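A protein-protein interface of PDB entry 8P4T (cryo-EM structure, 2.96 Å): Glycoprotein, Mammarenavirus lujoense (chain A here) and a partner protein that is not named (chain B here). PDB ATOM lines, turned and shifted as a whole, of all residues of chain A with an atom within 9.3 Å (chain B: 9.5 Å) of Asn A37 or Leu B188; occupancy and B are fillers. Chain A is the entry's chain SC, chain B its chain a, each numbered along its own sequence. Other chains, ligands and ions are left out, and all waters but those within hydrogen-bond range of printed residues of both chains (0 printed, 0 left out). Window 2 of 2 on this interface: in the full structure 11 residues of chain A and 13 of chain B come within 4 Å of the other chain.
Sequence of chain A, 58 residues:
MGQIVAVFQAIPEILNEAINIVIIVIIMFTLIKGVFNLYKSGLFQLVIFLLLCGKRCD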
ATOM      1  N   THR A  30     -14.074  -9.573  -4.851  1.00  0.00           N
ATOM      2  CA  THR A  30     -13.922 -11.017  -4.691  1.00  0.00           C
ATOM      3  C   THR A  30     -12.501 -11.460  -5.017  1.00  0.00           C
ATOM      4  O   THR A  30     -11.921 -12.285  -4.300  1.00  0.00           O
ATOM      5  CB  THR A  30     -14.929 -11.753  -5.574  1.00  0.00           C
ATOM      6  OG1 THR A  30     -16.203 -11.103  -5.495  1.00  0.00           O
ATOM      7  CG2 THR A  30     -15.075 -13.197  -5.121  1.00  0.00           C
ATOM      8  N   LEU A  31     -11.928 -10.932  -6.102  1.00  0.00           N
ATOM      9  CA  LEU A  31     -10.537 -11.227  -6.426  1.00  0.00           C
ATOM     10  C   LEU A  31      -9.591 -10.751  -5.330  1.00  0.00           C
ATOM     11  O   LEU A  31      -8.565 -11.392  -5.075  1.00  0.00           O
ATOM     12  CB  LEU A  31     -10.161 -10.588  -7.763  1.00  0.00           C
ATOM     13  CG  LEU A  31     -10.653 -11.304  -9.023  1.00  0.00           C
ATOM     14  CD1 LEU A  31     -10.563 -10.384 -10.231  1.00  0.00           C
ATOM     15  CD2 LEU A  31      -9.859 -12.579  -9.256  1.00  0.00           C
ATOM     16  N   ILE A  32      -9.914  -9.632  -4.678  1.00  0.00           N
ATOM     17  CA  ILE A  32      -9.053  -9.107  -3.622  1.00  0.00           C
ATOM     18  C   ILE A  32      -9.018 -10.062  -2.434  1.00  0.00           C
ATOM     19  O   ILE A  32      -7.961 -10.289  -1.833  1.00  0.00           O
ATOM     20  CB  ILE A  32      -9.520  -7.699  -3.207  1.00  0.00           C
ATOM     21  CG1 ILE A  32      -9.325  -6.713  -4.360  1.00  0.00           C
ATOM     22  CG2 ILE A  32      -8.773  -7.224  -1.972  1.00  0.00           C
ATOM     23  CD1 ILE A  32      -7.884  -6.562  -4.798  1.00  0.00           C
ATOM     24  N   LYS A  33     -10.169 -10.643  -2.081  1.00  0.00           N
ATOM     25  CA  LYS A  33     -10.196 -11.634  -1.009  1.00  0.00           C
ATOM     26  C   LYS A  33      -9.396 -12.875  -1.388  1.00  0.00           C
ATOM     27  O   LYS A  33      -8.733 -13.480  -0.537  1.00  0.00           O
ATOM     28  CB  LYS A  33     -11.641 -12.004  -0.674  1.00  0.00           C
ATOM     29  CG  LYS A  33     -11.788 -13.094   0.379  1.00  0.00           C
ATOM     30  CD  LYS A  33     -11.017 -12.758   1.646  1.00  0.00           C
ATOM     31  CE  LYS A  33     -10.664 -14.012   2.428  1.00  0.00           C
ATOM     32  NZ  LYS A  33      -9.741 -14.898   1.668  1.00  0.00           N
ATOM     33  N   GLY A  34      -9.449 -13.270  -2.661  1.00  0.00           N
ATOM     34  CA  GLY A  34      -8.608 -14.364  -3.122  1.00  0.00           C
ATOM     35  C   GLY A  34      -7.129 -14.078  -2.948  1.00  0.00           C
ATOM     36  O   GLY A  34      -6.361 -14.953  -2.540  1.00  0.00           O
ATOM     37  N   VAL A  35      -6.707 -12.851  -3.262  1.00  0.00           N
ATOM     38  CA  VAL A  35      -5.315 -12.462  -3.051  1.00  0.00           C
ATOM     39  C   VAL A  35      -4.966 -12.508  -1.568  1.00  0.00           C
ATOM     40  O   VAL A  35      -3.848 -12.880  -1.189  1.00  0.00           O
ATOM     41  CB  VAL A  35      -5.054 -11.069  -3.656  1.00  0.00           C
ATOM     42  CG1 VAL A  35      -3.644 -10.595  -3.336  1.00  0.00           C
ATOM     43  CG2 VAL A  35      -5.284 -11.093  -5.159  1.00  0.00           C
ATOM     44  N   PHE A  36      -5.916 -12.136  -0.706  1.00  0.00           N
ATOM     45  CA  PHE A  36      -5.652 -12.124   0.730  1.00  0.00           C
ATOM     46  C   PHE A  36      -5.349 -13.525   1.251  1.00  0.00           C
ATOM     47  O   PHE A  36      -4.470 -13.700   2.103  1.00  0.00           O
ATOM     48  CB  PHE A  36      -6.839 -11.519   1.480  1.00  0.00           C
ATOM     49  CG  PHE A  36      -6.923 -10.022   1.380  1.00  0.00           C
ATOM     50  CD1 PHE A  36      -5.837  -9.280   0.942  1.00  0.00           C
ATOM     51  CD2 PHE A  36      -8.086  -9.356   1.728  1.00  0.00           C
ATOM     52  CE1 PHE A  36      -5.913  -7.903   0.851  1.00  0.00           C
ATOM     53  CE2 PHE A  36      -8.168  -7.980   1.640  1.00  0.00           C
ATOM     54  CZ  PHE A  36      -7.079  -7.252   1.201  1.00  0.00           C
ATOM     55  N   ASN A  37      -6.078 -14.531   0.761  1.00  0.00           N
ATOM     56  CA  ASN A  37      -5.791 -15.911   1.142  1.00  0.00           C
ATOM     57  C   ASN A  37      -4.370 -16.305   0.754  1.00  0.00           C
ATOM     58  O   ASN A  37      -3.633 -16.887   1.558  1.00  0.00           O
ATOM     59  CB  ASN A  37      -6.809 -16.853   0.499  1.00  0.00           C
ATOM     60  CG  ASN A  37      -6.705 -18.270   1.027  1.00  0.00           C
ATOM     61  OD1 ASN A  37      -6.121 -18.511   2.084  1.00  0.00           O
ATOM     62  ND2 ASN A  37      -7.273 -19.219   0.291  1.00  0.00           N
ATOM     63  N   LEU A  38      -3.977 -16.008  -0.483  1.00  0.00           N
ATOM     64  CA  LEU A  38      -2.643 -16.337  -0.982  1.00  0.00           C
ATOM     65  C   LEU A  38      -1.545 -15.731  -0.111  1.00  0.00           C
ATOM     66  O   LEU A  38      -0.819 -16.447   0.578  1.00  0.00           O
ATOM     67  CB  LEU A  38      -2.480 -15.864  -2.430  1.00  0.00           C
ATOM     68  CG  LEU A  38      -2.839 -16.851  -3.546  1.00  0.00           C
ATOM     69  CD1 LEU A  38      -1.889 -18.040  -3.535  1.00  0.00           C
ATOM     70  CD2 LEU A  38      -4.285 -17.316  -3.447  1.00  0.00           C
ATOM     71  N   PHE B 181     -15.244 -19.524  -7.385  1.00  0.00           N
ATOM     72  CA  PHE B 181     -13.877 -19.560  -6.879  1.00  0.00           C
ATOM     73  C   PHE B 181     -13.742 -18.868  -5.528  1.00  0.00           C
ATOM     74  O   PHE B 181     -12.765 -19.118  -4.823  1.00  0.00           O
ATOM     75  CB  PHE B 181     -12.891 -18.980  -7.910  1.00  0.00           C
ATOM     76  CG  PHE B 181     -12.723 -17.480  -7.864  1.00  0.00           C
ATOM     77  CD1 PHE B 181     -11.873 -16.883  -6.941  1.00  0.00           C
ATOM     78  CD2 PHE B 181     -13.366 -16.673  -8.785  1.00  0.00           C
ATOM     79  CE1 PHE B 181     -11.708 -15.513  -6.912  1.00  0.00           C
ATOM     80  CE2 PHE B 181     -13.198 -15.299  -8.761  1.00  0.00           C
ATOM     81  CZ  PHE B 181     -12.370 -14.721  -7.823  1.00  0.00           C
ATOM     82  N   TYR B 182     -14.722 -18.060  -5.116  1.00  0.00           N
ATOM     83  CA  TYR B 182     -14.746 -17.591  -3.735  1.00  0.00           C
ATOM     84  C   TYR B 182     -15.071 -18.732  -2.781  1.00  0.00           C
ATOM     85  O   TYR B 182     -14.476 -18.840  -1.700  1.00  0.00           O
ATOM     86  CB  TYR B 182     -15.756 -16.452  -3.586  1.00  0.00           C
ATOM     87  CG  TYR B 182     -16.228 -16.223  -2.167  1.00  0.00           C
ATOM     88  CD1 TYR B 182     -15.481 -15.457  -1.281  1.00  0.00           C
ATOM     89  CD2 TYR B 182     -17.426 -16.765  -1.715  1.00  0.00           C
ATOM     90  CE1 TYR B 182     -15.910 -15.243   0.015  1.00  0.00           C
ATOM     91  CE2 TYR B 182     -17.860 -16.560  -0.420  1.00  0.00           C
ATOM     92  CZ  TYR B 182     -17.100 -15.797   0.440  1.00  0.00           C
ATOM     93  OH  TYR B 182     -17.532 -15.588   1.728  1.00  0.00           O
ATOM     94  N   MET B 183     -16.012 -19.597  -3.168  1.00  0.00           N
ATOM     95  CA  MET B 183     -16.244 -20.827  -2.419  1.00  0.00           C
ATOM     96  C   MET B 183     -14.993 -21.694  -2.396  1.00  0.00           C
ATOM     97  O   MET B 183     -14.651 -22.276  -1.360  1.00  0.00           O
ATOM     98  CB  MET B 183     -17.420 -21.596  -3.020  1.00  0.00           C
ATOM     99  CG  MET B 183     -18.763 -20.899  -2.866  1.00  0.00           C
ATOM    100  SD  MET B 183     -20.156 -21.932  -3.360  1.00  0.00           S
ATOM    101  CE  MET B 183     -20.223 -21.592  -5.117  1.00  0.00           C
ATOM    102  N   PHE B 184     -14.304 -21.799  -3.535  1.00  0.00           N
ATOM    103  CA  PHE B 184     -13.042 -22.535  -3.574  1.00  0.00           C
ATOM    104  C   PHE B 184     -12.018 -21.937  -2.612  1.00  0.00           C
ATOM    105  O   PHE B 184     -11.275 -22.669  -1.949  1.00  0.00           O
ATOM    106  CB  PHE B 184     -12.485 -22.550  -4.999  1.00  0.00           C
ATOM    107  CG  PHE B 184     -13.335 -23.311  -5.977  1.00  0.00           C
ATOM    108  CD1 PHE B 184     -14.214 -24.288  -5.543  1.00  0.00           C
ATOM    109  CD2 PHE B 184     -13.250 -23.050  -7.335  1.00  0.00           C
ATOM    110  CE1 PHE B 184     -14.995 -24.988  -6.442  1.00  0.00           C
ATOM    111  CE2 PHE B 184     -14.029 -23.746  -8.240  1.00  0.00           C
ATOM    112  CZ  PHE B 184     -14.902 -24.717  -7.793  1.00  0.00           C
ATOM    113  N   SER B 185     -11.957 -20.606  -2.536  1.00  0.00           N
ATOM    114  CA  SER B 185     -10.992 -19.940  -1.669  1.00  0.00           C
ATOM    115  C   SER B 185     -11.300 -20.200  -0.199  1.00  0.00           C
ATOM    116  O   SER B 185     -10.416 -20.593   0.571  1.00  0.00           O
ATOM    117  CB  SER B 185     -10.976 -18.439  -1.959  1.00  0.00           C
ATOM    118  OG  SER B 185     -10.252 -17.734  -0.965  1.00  0.00           O
ATOM    119  N   VAL B 186     -12.553 -19.983   0.209  1.00  0.00           N
ATOM    120  CA  VAL B 186     -12.918 -20.192   1.607  1.00  0.00           C
ATOM    121  C   VAL B 186     -12.941 -21.676   1.959  1.00  0.00           C
ATOM    122  O   VAL B 186     -12.933 -22.031   3.144  1.00  0.00           O
ATOM    123  CB  VAL B 186     -14.271 -19.519   1.913  1.00  0.00           C
ATOM    124  CG1 VAL B 186     -14.522 -19.455   3.414  1.00  0.00           C
ATOM    125  CG2 VAL B 186     -14.305 -18.121   1.328  1.00  0.00           C
ATOM    126  N   THR B 187     -12.954 -22.559   0.956  1.00  0.00           N
ATOM    127  CA  THR B 187     -12.812 -23.987   1.218  1.00  0.00           C
ATOM    128  C   THR B 187     -11.504 -24.297   1.936  1.00  0.00           C
ATOM    129  O   THR B 187     -11.454 -25.201   2.777  1.00  0.00           O
ATOM    130  CB  THR B 187     -12.901 -24.769  -0.095  1.00  0.00           C
ATOM    131  OG1 THR B 187     -14.157 -24.498  -0.732  1.00  0.00           O
ATOM    132  CG2 THR B 187     -12.777 -26.267   0.149  1.00  0.00           C
ATOM    133  N   LEU B 188     -10.447 -23.548   1.638  1.00  0.00           N
ATOM    134  CA  LEU B 188      -9.162 -23.732   2.300  1.00  0.00           C
ATOM    135  C   LEU B 188      -9.194 -23.177   3.719  1.00  0.00           C
ATOM    136  O   LEU B 188     -10.120 -22.458   4.094  1.00  0.00           O
ATOM    137  CB  LEU B 188      -8.045 -23.058   1.498  1.00  0.00           C
ATOM    138  CG  LEU B 188      -7.836 -23.547   0.064  1.00  0.00           C
ATOM    139  CD1 LEU B 188      -6.568 -22.950  -0.527  1.00  0.00           C
ATOM    140  CD2 LEU B 188      -7.790 -25.067   0.013  1.00  0.00           C
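Asn A37 touches just these residues of chain B: Ser B185 (3.4 Å) and Leu B188 (3.9 Å).
Of the printed residues of chain A, Leu B188 touches Asn A37 (3.9 Å).
No residue of chain B comes within 4 Å of Gly A34.
No residue of chain B comes within 4 Å of Leu A38.
Of the printed residues of chain A, Phe B181 touches Leu A31 (3.6 Å).
Of the printed residues of chain A, Tyr B182 touches Thr A30.
Ile A32 touches none of the printed residues of chain B.
Phe A36 touches none of the printed residues of chain B.
The nearest residue of chain B that does not touch Asn A37 is Val B186 (5.3 Å).
The nearest residue of chain A that does not touch Leu B188 is Leu A38 (6.7 Å).
The nearest printed residue of chain B that does not touch Thr A30 is Phe B181 (4.1 Å).
The backbone carbonyl oxygen of Ser B185 is in hydrogen-bond range of the side-chain amide nitrogen of Asn A37 (3.4 Å).
Of the 9 printed residues of chain A, 4 touch a printed residue of chain B.
Hydrophobic or aromatic side chains of chain A that line the printed part of chain B: Leu A31.
Of the 8 printed residues of chain B, 4 touch a printed residue of chain A.
Hydrophobic or aromatic side chains of chain B within 4 Å of the printed part of chain A: Phe B181, Tyr B182 and Leu B188.
Among the printed residues, no Asp or Glu carboxylate lies within 4 Å of a Lys or Arg side-chain nitrogen of the other chain.
Tyr B182 touches Thr A30.
CD2 of Leu A31 touches CZ of Phe B181, 3.6 Å away.
OG of Ser B185 touches NZ of Lys A33, 3.9 Å away.
ND2 of Asn A37 touches CD1 of Leu B188, at 3.9 Å.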
